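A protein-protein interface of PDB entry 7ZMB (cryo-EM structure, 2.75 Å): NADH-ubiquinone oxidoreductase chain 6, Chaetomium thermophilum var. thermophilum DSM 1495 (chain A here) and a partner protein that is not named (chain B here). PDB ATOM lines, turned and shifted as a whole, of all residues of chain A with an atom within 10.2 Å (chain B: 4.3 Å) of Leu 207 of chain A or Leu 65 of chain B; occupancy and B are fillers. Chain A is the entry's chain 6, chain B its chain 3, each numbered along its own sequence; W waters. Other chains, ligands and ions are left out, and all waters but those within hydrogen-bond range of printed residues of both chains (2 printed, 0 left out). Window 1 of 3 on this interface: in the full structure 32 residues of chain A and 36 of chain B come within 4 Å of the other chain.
SD of Met 211 of chain A sits close to OE2 of Glu 69 of chain B.
Leu 68 of chain B touches Val 76 of chain A.
CE2 of Phe 63 of chain B touches O of Gly 79 of chain A (3.7 Å).
Ala 80 of chain A touches Leu 64 of chain B.
CD1 of Leu 64 of chain B touches CG2 of Ile 83 of chain A (3.8 Å).
Leu 65 of chain B touches Leu 207 of chain A (O to CD2, 3.9 Å).
Leu 68 of chain B touches Leu 207 of chain A (CD1 to CD2, 3.9 Å).
Glu 69 of chain B touches Leu 207 of chain A.
CD2 of Leu 65 of chain B touches CB of Ala 210 of chain A (3.9 Å).
Met 211 of chain A touches Leu 65 of chain B.
Ile 215 of chain A touches Val 62 of chain B (CD1 to CG1, 3.8 Å).
Leu 207 of chain A touches just these residues of chain B: Leu 65, Leu 68 and Glu 69.
Leu 65 of chain B touches just these residues of chain A: Leu 207, Ala 210 and Met 211.
No residue of chain A comes within 4 Å of Leu 66 of chain B.
Leu 68 of chain B touches just these residues of chain A: Val 76 (3.8 Å) and Leu 207 (3.9 Å).
Of the printed residues of chain B, Ile 83 of chain A touches Phe 63 (3.7 Å) and Leu 64 (3.8 Å).
Printed residues of chain B within 4 Å of Ile 215 of chain A: Val 62 (3.8 Å).
Of the printed residues of chain B, Ala 210 of chain A touches Leu 65.
Phe 205 of chain A touches none of the printed residues of chain B.
Ser 204 of chain A touches none of the printed residues of chain B.
The nearest printed residue of chain A that does not touch Val 62 of chain B is Met 211 of chain A (5.3 Å).
Hydrophobic or aromatic side chains of chain A within 4 Å of the printed part of chain B: Val 76, Ala 80, Ile 83, Leu 207, Ala 210, Met 211 and Ile 215.
Printed residues of chain B that touch a printed residue of chain A: Val 62, Phe 63, Leu 64, Leu 65, Leu 68 and Glu 69.
Hydrophobic or aromatic side chains of chain B that line the printed part of chain A: Val 62, Phe 63, Leu 64, Leu 65 and Leu 68.
Along chain B the printed residues that touch a printed residue of chain A span positions 62 to 69.
Among the printed residues, 12 pairs touch across the chains.
Water W2 lies within hydrogen-bond range of the backbone carbonyl oxygen of Val 76 of chain A (2.6 Å), the side-chain carboxylate of Asp 67 of chain B (3.0 Å) and the backbone NH of Ala 80 of chain A (3.5 Å).
Water W1 bridges O of Val 62 of chain B and SD of Met 211 of chain A.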
ATOM      1  N   VAL A  76      13.143  33.094  15.152  1.00  0.00           N
ATOM      2  CA  VAL A  76      12.353  32.542  16.284  1.00  0.00           C
ATOM      3  C   VAL A  76      13.228  32.442  17.538  1.00  0.00           C
ATOM      4  O   VAL A  76      12.716  32.713  18.623  1.00  0.00           O
ATOM      5  CB  VAL A  76      11.677  31.218  15.872  1.00  0.00           C
ATOM      6  CG1 VAL A  76      11.521  30.257  17.039  1.00  0.00           C
ATOM      7  CG2 VAL A  76      10.342  31.471  15.198  1.00  0.00           C
ATOM      8  N   GLY A  79      13.863  36.157  19.372  1.00  0.00           N
ATOM      9  CA  GLY A  79      12.740  36.461  20.242  1.00  0.00           C
ATOM     10  C   GLY A  79      12.665  35.544  21.445  1.00  0.00           C
ATOM     11  O   GLY A  79      12.341  35.979  22.549  1.00  0.00           O
ATOM     12  N   ALA A  80      12.970  34.261  21.251  1.00  0.00           N
ATOM     13  CA  ALA A  80      12.943  33.320  22.366  1.00  0.00           C
ATOM     14  C   ALA A  80      14.036  33.623  23.379  1.00  0.00           C
ATOM     15  O   ALA A  80      13.797  33.569  24.590  1.00  0.00           O
ATOM     16  CB  ALA A  80      13.071  31.887  21.853  1.00  0.00           C
ATOM     17  N   ILE A  83      13.196  36.615  25.478  1.00  0.00           N
ATOM     18  CA  ILE A  83      12.240  36.278  26.525  1.00  0.00           C
ATOM     19  C   ILE A  83      12.930  35.524  27.653  1.00  0.00           C
ATOM     20  O   ILE A  83      12.634  35.737  28.834  1.00  0.00           O
ATOM     21  CB  ILE A  83      11.063  35.483  25.931  1.00  0.00           C
ATOM     22  CG1 ILE A  83      10.260  36.366  24.975  1.00  0.00           C
ATOM     23  CG2 ILE A  83      10.165  34.928  27.023  1.00  0.00           C
ATOM     24  CD1 ILE A  83       9.988  37.746  25.514  1.00  0.00           C
ATOM     25  N   TRP A 199      -0.133  17.149  10.515  1.00  0.00           N
ATOM     26  CA  TRP A 199       0.952  17.662  11.380  1.00  0.00           C
ATOM     27  C   TRP A 199       0.651  19.108  11.728  1.00  0.00           C
ATOM     28  O   TRP A 199       0.900  19.475  12.866  1.00  0.00           O
ATOM     29  CB  TRP A 199       2.326  17.531  10.716  1.00  0.00           C
ATOM     30  CG  TRP A 199       2.756  16.130  10.418  1.00  0.00           C
ATOM     31  CD1 TRP A 199       2.270  14.976  10.960  1.00  0.00           C
ATOM     32  CD2 TRP A 199       3.797  15.739   9.508  1.00  0.00           C
ATOM     33  NE1 TRP A 199       2.931  13.896  10.443  1.00  0.00           N
ATOM     34  CE2 TRP A 199       3.873  14.331   9.551  1.00  0.00           C
ATOM     35  CE3 TRP A 199       4.665  16.439   8.664  1.00  0.00           C
ATOM     36  CZ2 TRP A 199       4.784  13.614   8.779  1.00  0.00           C
ATOM     37  CZ3 TRP A 199       5.564  15.729   7.904  1.00  0.00           C
ATOM     38  CH2 TRP A 199       5.621  14.337   7.964  1.00  0.00           C
ATOM     39  N   LEU A 200       0.122  19.878  10.776  1.00  0.00           N
ATOM     40  CA  LEU A 200      -0.269  21.250  11.074  1.00  0.00           C
ATOM     41  C   LEU A 200      -1.406  21.298  12.087  1.00  0.00           C
ATOM     42  O   LEU A 200      -1.404  22.141  12.988  1.00  0.00           O
ATOM     43  CB  LEU A 200      -0.662  21.963   9.787  1.00  0.00           C
ATOM     44  CG  LEU A 200      -1.038  23.438   9.881  1.00  0.00           C
ATOM     45  CD1 LEU A 200       0.176  24.271  10.153  1.00  0.00           C
ATOM     46  CD2 LEU A 200      -1.700  23.876   8.595  1.00  0.00           C
ATOM     47  N   ILE A 201      -2.385  20.404  11.956  1.00  0.00           N
ATOM     48  CA  ILE A 201      -3.520  20.414  12.870  1.00  0.00           C
ATOM     49  C   ILE A 201      -3.083  20.003  14.272  1.00  0.00           C
ATOM     50  O   ILE A 201      -3.445  20.647  15.261  1.00  0.00           O
ATOM     51  CB  ILE A 201      -4.655  19.528  12.326  1.00  0.00           C
ATOM     52  CG1 ILE A 201      -5.160  20.084  11.003  1.00  0.00           C
ATOM     53  CG2 ILE A 201      -5.807  19.515  13.274  1.00  0.00           C
ATOM     54  CD1 ILE A 201      -5.984  19.138  10.206  1.00  0.00           C
ATOM     55  N   LEU A 202      -2.275  18.945  14.378  1.00  0.00           N
ATOM     56  CA  LEU A 202      -1.703  18.576  15.670  1.00  0.00           C
ATOM     57  C   LEU A 202      -0.808  19.672  16.226  1.00  0.00           C
ATOM     58  O   LEU A 202      -0.869  19.984  17.419  1.00  0.00           O
ATOM     59  CB  LEU A 202      -0.925  17.264  15.561  1.00  0.00           C
ATOM     60  CG  LEU A 202      -1.626  15.912  15.654  1.00  0.00           C
ATOM     61  CD1 LEU A 202      -2.226  15.748  17.030  1.00  0.00           C
ATOM     62  CD2 LEU A 202      -2.710  15.755  14.605  1.00  0.00           C
ATOM     63  N   ALA A 203       0.050  20.246  15.386  1.00  0.00           N
ATOM     64  CA  ALA A 203       0.926  21.362  15.817  1.00  0.00           C
ATOM     65  C   ALA A 203       0.077  22.441  16.484  1.00  0.00           C
ATOM     66  O   ALA A 203       0.471  22.939  17.550  1.00  0.00           O
ATOM     67  CB  ALA A 203       1.744  21.886  14.676  1.00  0.00           C
ATOM     68  N   SER A 204      -1.018  22.814  15.820  1.00  0.00           N
ATOM     69  CA  SER A 204      -1.913  23.888  16.302  1.00  0.00           C
ATOM     70  C   SER A 204      -2.484  23.547  17.677  1.00  0.00           C
ATOM     71  O   SER A 204      -2.618  24.468  18.493  1.00  0.00           O
ATOM     72  CB  SER A 204      -3.007  24.112  15.297  1.00  0.00           C
ATOM     73  OG  SER A 204      -4.047  23.164  15.445  1.00  0.00           O
ATOM     74  N   PHE A 205      -2.834  22.281  17.905  1.00  0.00           N
ATOM     75  CA  PHE A 205      -3.359  21.847  19.223  1.00  0.00           C
ATOM     76  C   PHE A 205      -2.286  21.991  20.313  1.00  0.00           C
ATOM     77  O   PHE A 205      -2.634  22.379  21.437  1.00  0.00           O
ATOM     78  CB  PHE A 205      -4.119  20.519  19.113  1.00  0.00           C
ATOM     79  CG  PHE A 205      -5.590  20.709  18.842  1.00  0.00           C
ATOM     80  CD1 PHE A 205      -6.032  21.177  17.617  1.00  0.00           C
ATOM     81  CD2 PHE A 205      -6.532  20.457  19.825  1.00  0.00           C
ATOM     82  CE1 PHE A 205      -7.382  21.375  17.376  1.00  0.00           C
ATOM     83  CE2 PHE A 205      -7.881  20.651  19.584  1.00  0.00           C
ATOM     84  CZ  PHE A 205      -8.305  21.107  18.359  1.00  0.00           C
ATOM     85  N   ILE A 206      -1.031  21.675  19.999  1.00  0.00           N
ATOM     86  CA  ILE A 206       0.077  21.819  20.992  1.00  0.00           C
ATOM     87  C   ILE A 206       0.226  23.300  21.346  1.00  0.00           C
ATOM     88  O   ILE A 206       0.327  23.608  22.546  1.00  0.00           O
ATOM     89  CB  ILE A 206       1.397  21.196  20.481  1.00  0.00           C
ATOM     90  CG1 ILE A 206       1.201  19.735  20.072  1.00  0.00           C
ATOM     91  CG2 ILE A 206       2.516  21.356  21.496  1.00  0.00           C
ATOM     92  CD1 ILE A 206       2.322  19.181  19.230  1.00  0.00           C
ATOM     93  N   LEU A 207       0.182  24.175  20.340  1.00  0.00           N
ATOM     94  CA  LEU A 207       0.299  25.637  20.572  1.00  0.00           C
ATOM     95  C   LEU A 207      -0.888  26.132  21.397  1.00  0.00           C
ATOM     96  O   LEU A 207      -0.664  26.944  22.297  1.00  0.00           O
ATOM     97  CB  LEU A 207       0.332  26.330  19.215  1.00  0.00           C
ATOM     98  CG  LEU A 207       1.600  26.132  18.400  1.00  0.00           C
ATOM     99  CD1 LEU A 207       1.267  26.177  16.924  1.00  0.00           C
ATOM    100  CD2 LEU A 207       2.642  27.177  18.764  1.00  0.00           C
ATOM    101  N   LEU A 208      -2.088  25.635  21.109  1.00  0.00           N
ATOM    102  CA  LEU A 208      -3.304  26.038  21.850  1.00  0.00           C
ATOM    103  C   LEU A 208      -3.178  25.636  23.320  1.00  0.00           C
ATOM    104  O   LEU A 208      -3.499  26.463  24.184  1.00  0.00           O
ATOM    105  CB  LEU A 208      -4.498  25.327  21.207  1.00  0.00           C
ATOM    106  CG  LEU A 208      -5.874  25.831  21.614  1.00  0.00           C
ATOM    107  CD1 LEU A 208      -6.017  27.289  21.231  1.00  0.00           C
ATOM    108  CD2 LEU A 208      -6.958  24.998  20.952  1.00  0.00           C
ATOM    109  N   LEU A 209      -2.726  24.415  23.584  1.00  0.00           N
ATOM    110  CA  LEU A 209      -2.575  23.947  24.977  1.00  0.00           C
ATOM    111  C   LEU A 209      -1.528  24.812  25.679  1.00  0.00           C
ATOM    112  O   LEU A 209      -1.785  25.220  26.819  1.00  0.00           O
ATOM    113  CB  LEU A 209      -2.209  22.460  24.954  1.00  0.00           C
ATOM    114  CG  LEU A 209      -1.635  21.859  26.233  1.00  0.00           C
ATOM    115  CD1 LEU A 209      -2.733  21.605  27.249  1.00  0.00           C
ATOM    116  CD2 LEU A 209      -0.900  20.568  25.917  1.00  0.00           C
ATOM    117  N   ALA A 210      -0.424  25.129  25.005  1.00  0.00           N
ATOM    118  CA  ALA A 210       0.599  26.021  25.597  1.00  0.00           C
ATOM    119  C   ALA A 210       0.033  27.427  25.846  1.00  0.00           C
ATOM    120  O   ALA A 210       0.322  27.983  26.906  1.00  0.00           O
ATOM    121  CB  ALA A 210       1.820  26.045  24.729  1.00  0.00           C
ATOM    122  N   MET A 211      -0.753  27.970  24.916  1.00  0.00           N
ATOM    123  CA  MET A 211      -1.384  29.310  25.078  1.00  0.00           C
ATOM    124  C   MET A 211      -2.370  29.289  26.253  1.00  0.00           C
ATOM    125  O   MET A 211      -2.425  30.282  26.980  1.00  0.00           O
ATOM    126  CB  MET A 211      -2.107  29.746  23.798  1.00  0.00           C
ATOM    127  CG  MET A 211      -1.192  30.011  22.626  1.00  0.00           C
ATOM    128  SD  MET A 211      -2.100  30.419  21.115  1.00  0.00           S
ATOM    129  CE  MET A 211      -2.667  32.073  21.504  1.00  0.00           C
ATOM    130  N   VAL A 212      -3.113  28.200  26.427  1.00  0.00           N
ATOM    131  CA  VAL A 212      -4.086  28.066  27.554  1.00  0.00           C
ATOM    132  C   VAL A 212      -3.358  27.642  28.831  1.00  0.00           C
ATOM    133  O   VAL A 212      -3.626  28.257  29.871  1.00  0.00           O
ATOM    134  CB  VAL A 212      -5.233  27.094  27.205  1.00  0.00           C
ATOM    135  CG1 VAL A 212      -6.111  26.775  28.405  1.00  0.00           C
ATOM    136  CG2 VAL A 212      -6.068  27.616  26.049  1.00  0.00           C
ATOM    137  N   GLY A 213      -2.468  26.650  28.761  1.00  0.00           N
ATOM    138  CA  GLY A 213      -1.842  26.164  29.977  1.00  0.00           C
ATOM    139  C   GLY A 213      -0.865  27.154  30.579  1.00  0.00           C
ATOM    140  O   GLY A 213      -0.866  27.382  31.789  1.00  0.00           O
ATOM    141  N   ALA A 214      -0.008  27.747  29.748  1.00  0.00           N
ATOM    142  CA  ALA A 214       0.995  28.666  30.273  1.00  0.00           C
ATOM    143  C   ALA A 214       0.363  29.886  30.924  1.00  0.00           C
ATOM    144  O   ALA A 214       1.016  30.556  31.726  1.00  0.00           O
ATOM    145  CB  ALA A 214       1.961  29.096  29.167  1.00  0.00           C
ATOM    146  N   ILE A 215      -0.901  30.148  30.614  1.00  0.00           N
ATOM    147  CA  ILE A 215      -1.605  31.340  31.162  1.00  0.00           C
ATOM    148  C   ILE A 215      -2.409  30.916  32.390  1.00  0.00           C
ATOM    149  O   ILE A 215      -2.473  31.701  33.341  1.00  0.00           O
ATOM    150  CB  ILE A 215      -2.475  31.990  30.068  1.00  0.00           C
ATOM    151  CG1 ILE A 215      -1.602  32.523  28.929  1.00  0.00           C
ATOM    152  CG2 ILE A 215      -3.386  33.066  30.637  1.00  0.00           C
ATOM    153  CD1 ILE A 215      -0.361  33.248  29.386  1.00  0.00           C
ATOM    154  N   VAL A 216      -2.968  29.704  32.378  1.00  0.00           N
ATOM    155  CA  VAL A 216      -3.786  29.209  33.524  1.00  0.00           C
ATOM    156  C   VAL A 216      -2.902  29.167  34.775  1.00  0.00           C
ATOM    157  O   VAL A 216      -3.406  29.519  35.850  1.00  0.00           O
ATOM    158  CB  VAL A 216      -4.483  27.863  33.236  1.00  0.00           C
ATOM    159  CG1 VAL A 216      -3.536  26.677  33.240  1.00  0.00           C
ATOM    160  CG2 VAL A 216      -5.622  27.611  34.205  1.00  0.00           C
ATOM    161  N   THR A 218      -0.097  30.971  35.467  1.00  0.00           N
ATOM    162  CA  THR A 218       0.660  32.195  35.844  1.00  0.00           C
ATOM    163  C   THR A 218      -0.226  33.436  35.861  1.00  0.00           C
ATOM    164  O   THR A 218       0.334  34.523  36.005  1.00  0.00           O
ATOM    165  CB  THR A 218       1.813  32.469  34.874  1.00  0.00           C
ATOM    166  OG1 THR A 218       1.252  32.679  33.579  1.00  0.00           O
ATOM    167  CG2 THR A 218       2.836  31.358  34.828  1.00  0.00           C
ATOM    168  N   LEU B  61       5.359  35.217  27.199  1.00  0.00           N
ATOM    169  CA  LEU B  61       5.008  33.827  26.941  1.00  0.00           C
ATOM    170  C   LEU B  61       4.123  33.702  25.709  1.00  0.00           C
ATOM    171  O   LEU B  61       4.361  32.848  24.850  1.00  0.00           O
ATOM    172  CB  LEU B  61       4.319  33.225  28.170  1.00  0.00           C
ATOM    173  CG  LEU B  61       5.171  32.964  29.413  1.00  0.00           C
ATOM    174  CD1 LEU B  61       4.321  32.770  30.652  1.00  0.00           C
ATOM    175  CD2 LEU B  61       6.055  31.763  29.203  1.00  0.00           C
ATOM    176  N   VAL B  62       3.090  34.542  25.600  1.00  0.00           N
ATOM    177  CA  VAL B  62       2.204  34.466  24.441  1.00  0.00           C
ATOM    178  C   VAL B  62       2.894  34.976  23.184  1.00  0.00           C
ATOM    179  O   VAL B  62       2.625  34.483  22.086  1.00  0.00           O
ATOM    180  CB  VAL B  62       0.874  35.201  24.705  1.00  0.00           C
ATOM    181  CG1 VAL B  62       0.287  34.771  26.012  1.00  0.00           C
ATOM    182  CG2 VAL B  62       1.068  36.699  24.703  1.00  0.00           C
ATOM    183  N   PHE B  63       3.786  35.963  23.313  1.00  0.00           N
ATOM    184  CA  PHE B  63       4.578  36.398  22.168  1.00  0.00           C
ATOM    185  C   PHE B  63       5.404  35.259  21.600  1.00  0.00           C
ATOM    186  O   PHE B  63       5.605  35.180  20.386  1.00  0.00           O
ATOM    187  CB  PHE B  63       5.495  37.552  22.567  1.00  0.00           C
ATOM    188  CG  PHE B  63       6.745  37.633  21.750  1.00  0.00           C
ATOM    189  CD1 PHE B  63       6.720  38.180  20.490  1.00  0.00           C
ATOM    190  CD2 PHE B  63       7.932  37.127  22.225  1.00  0.00           C
ATOM    191  CE1 PHE B  63       7.850  38.239  19.736  1.00  0.00           C
ATOM    192  CE2 PHE B  63       9.066  37.182  21.468  1.00  0.00           C
ATOM    193  CZ  PHE B  63       9.027  37.742  20.219  1.00  0.00           C
ATOM    194  N   LEU B  64       5.888  34.369  22.463  1.00  0.00           N
ATOM    195  CA  LEU B  64       6.700  33.239  22.033  1.00  0.00           C
ATOM    196  C   LEU B  64       5.939  32.353  21.058  1.00  0.00           C
ATOM    197  O   LEU B  64       6.487  31.938  20.033  1.00  0.00           O
ATOM    198  CB  LEU B  64       7.127  32.425  23.252  1.00  0.00           C
ATOM    199  CG  LEU B  64       8.419  32.715  24.007  1.00  0.00           C
ATOM    200  CD1 LEU B  64       8.335  32.069  25.362  1.00  0.00           C
ATOM    201  CD2 LEU B  64       9.630  32.216  23.282  1.00  0.00           C
ATOM    202  N   LEU B  65       4.687  32.038  21.392  1.00  0.00           N
ATOM    203  CA  LEU B  65       3.882  31.089  20.581  1.00  0.00           C
ATOM    204  C   LEU B  65       3.226  31.745  19.362  1.00  0.00           C
ATOM    205  O   LEU B  65       3.035  31.025  18.377  1.00  0.00           O
ATOM    206  CB  LEU B  65       2.827  30.481  21.504  1.00  0.00           C
ATOM    207  CG  LEU B  65       3.364  29.937  22.825  1.00  0.00           C
ATOM    208  CD1 LEU B  65       2.284  29.938  23.893  1.00  0.00           C
ATOM    209  CD2 LEU B  65       3.952  28.547  22.645  1.00  0.00           C
ATOM    210  N   LEU B  66       2.922  33.043  19.386  1.00  0.00           N
ATOM    211  CA  LEU B  66       2.204  33.616  18.217  1.00  0.00           C
ATOM    212  C   LEU B  66       3.243  33.866  17.132  1.00  0.00           C
ATOM    213  O   LEU B  66       2.855  33.926  15.960  1.00  0.00           O
ATOM    214  CB  LEU B  66       1.431  34.873  18.620  1.00  0.00           C
ATOM    215  CG  LEU B  66      -0.018  34.633  19.043  1.00  0.00           C
ATOM    216  CD1 LEU B  66      -0.623  35.877  19.656  1.00  0.00           C
ATOM    217  CD2 LEU B  66      -0.857  34.186  17.863  1.00  0.00           C
ATOM    218  N   ASP B  67       4.513  33.978  17.511  1.00  0.00           N
ATOM    219  CA  ASP B  67       5.611  34.064  16.516  1.00  0.00           C
ATOM    220  C   ASP B  67       5.680  32.740  15.751  1.00  0.00           C
ATOM    221  O   ASP B  67       5.822  32.783  14.530  1.00  0.00           O
ATOM    222  CB  ASP B  67       6.930  34.319  17.242  1.00  0.00           C
ATOM    223  CG  ASP B  67       8.038  34.928  16.403  1.00  0.00           C
ATOM    224  OD1 ASP B  67       7.869  35.020  15.174  1.00  0.00           O
ATOM    225  OD2 ASP B  67       9.066  35.314  16.994  1.00  0.00           O
ATOM    226  N   LEU B  68       5.607  31.615  16.457  1.00  0.00           N
ATOM    227  CA  LEU B  68       5.650  30.279  15.812  1.00  0.00           C
ATOM    228  C   LEU B  68       4.460  30.178  14.862  1.00  0.00           C
ATOM    229  O   LEU B  68       4.637  29.652  13.749  1.00  0.00           O
ATOM    230  CB  LEU B  68       5.567  29.221  16.908  1.00  0.00           C
ATOM    231  CG  LEU B  68       6.696  29.246  17.937  1.00  0.00           C
ATOM    232  CD1 LEU B  68       6.354  28.389  19.144  1.00  0.00           C
ATOM    233  CD2 LEU B  68       8.008  28.798  17.320  1.00  0.00           C
ATOM    234  N   GLU B  69       3.312  30.712  15.274  1.00  0.00           N
ATOM    235  CA  GLU B  69       2.079  30.667  14.453  1.00  0.00           C
ATOM    236  C   GLU B  69       2.185  31.480  13.155  1.00  0.00           C
ATOM    237  O   GLU B  69       1.687  30.985  12.130  1.00  0.00           O
ATOM    238  CB  GLU B  69       0.891  30.980  15.358  1.00  0.00           C
ATOM    239  CG  GLU B  69       0.567  29.812  16.273  1.00  0.00           C
ATOM    240  CD  GLU B  69      -0.020  30.120  17.640  1.00  0.00           C
ATOM    241  OE1 GLU B  69       0.029  31.283  18.053  1.00  0.00           O
ATOM    242  OE2 GLU B  69      -0.533  29.189  18.285  1.00  0.00           O
HETATM  243  O   HOH W   1       0.552  32.775  22.109  1.00  0.00           O
HETATM  244  O   HOH W   2      10.304  33.554  19.101  1.00  0.00           O
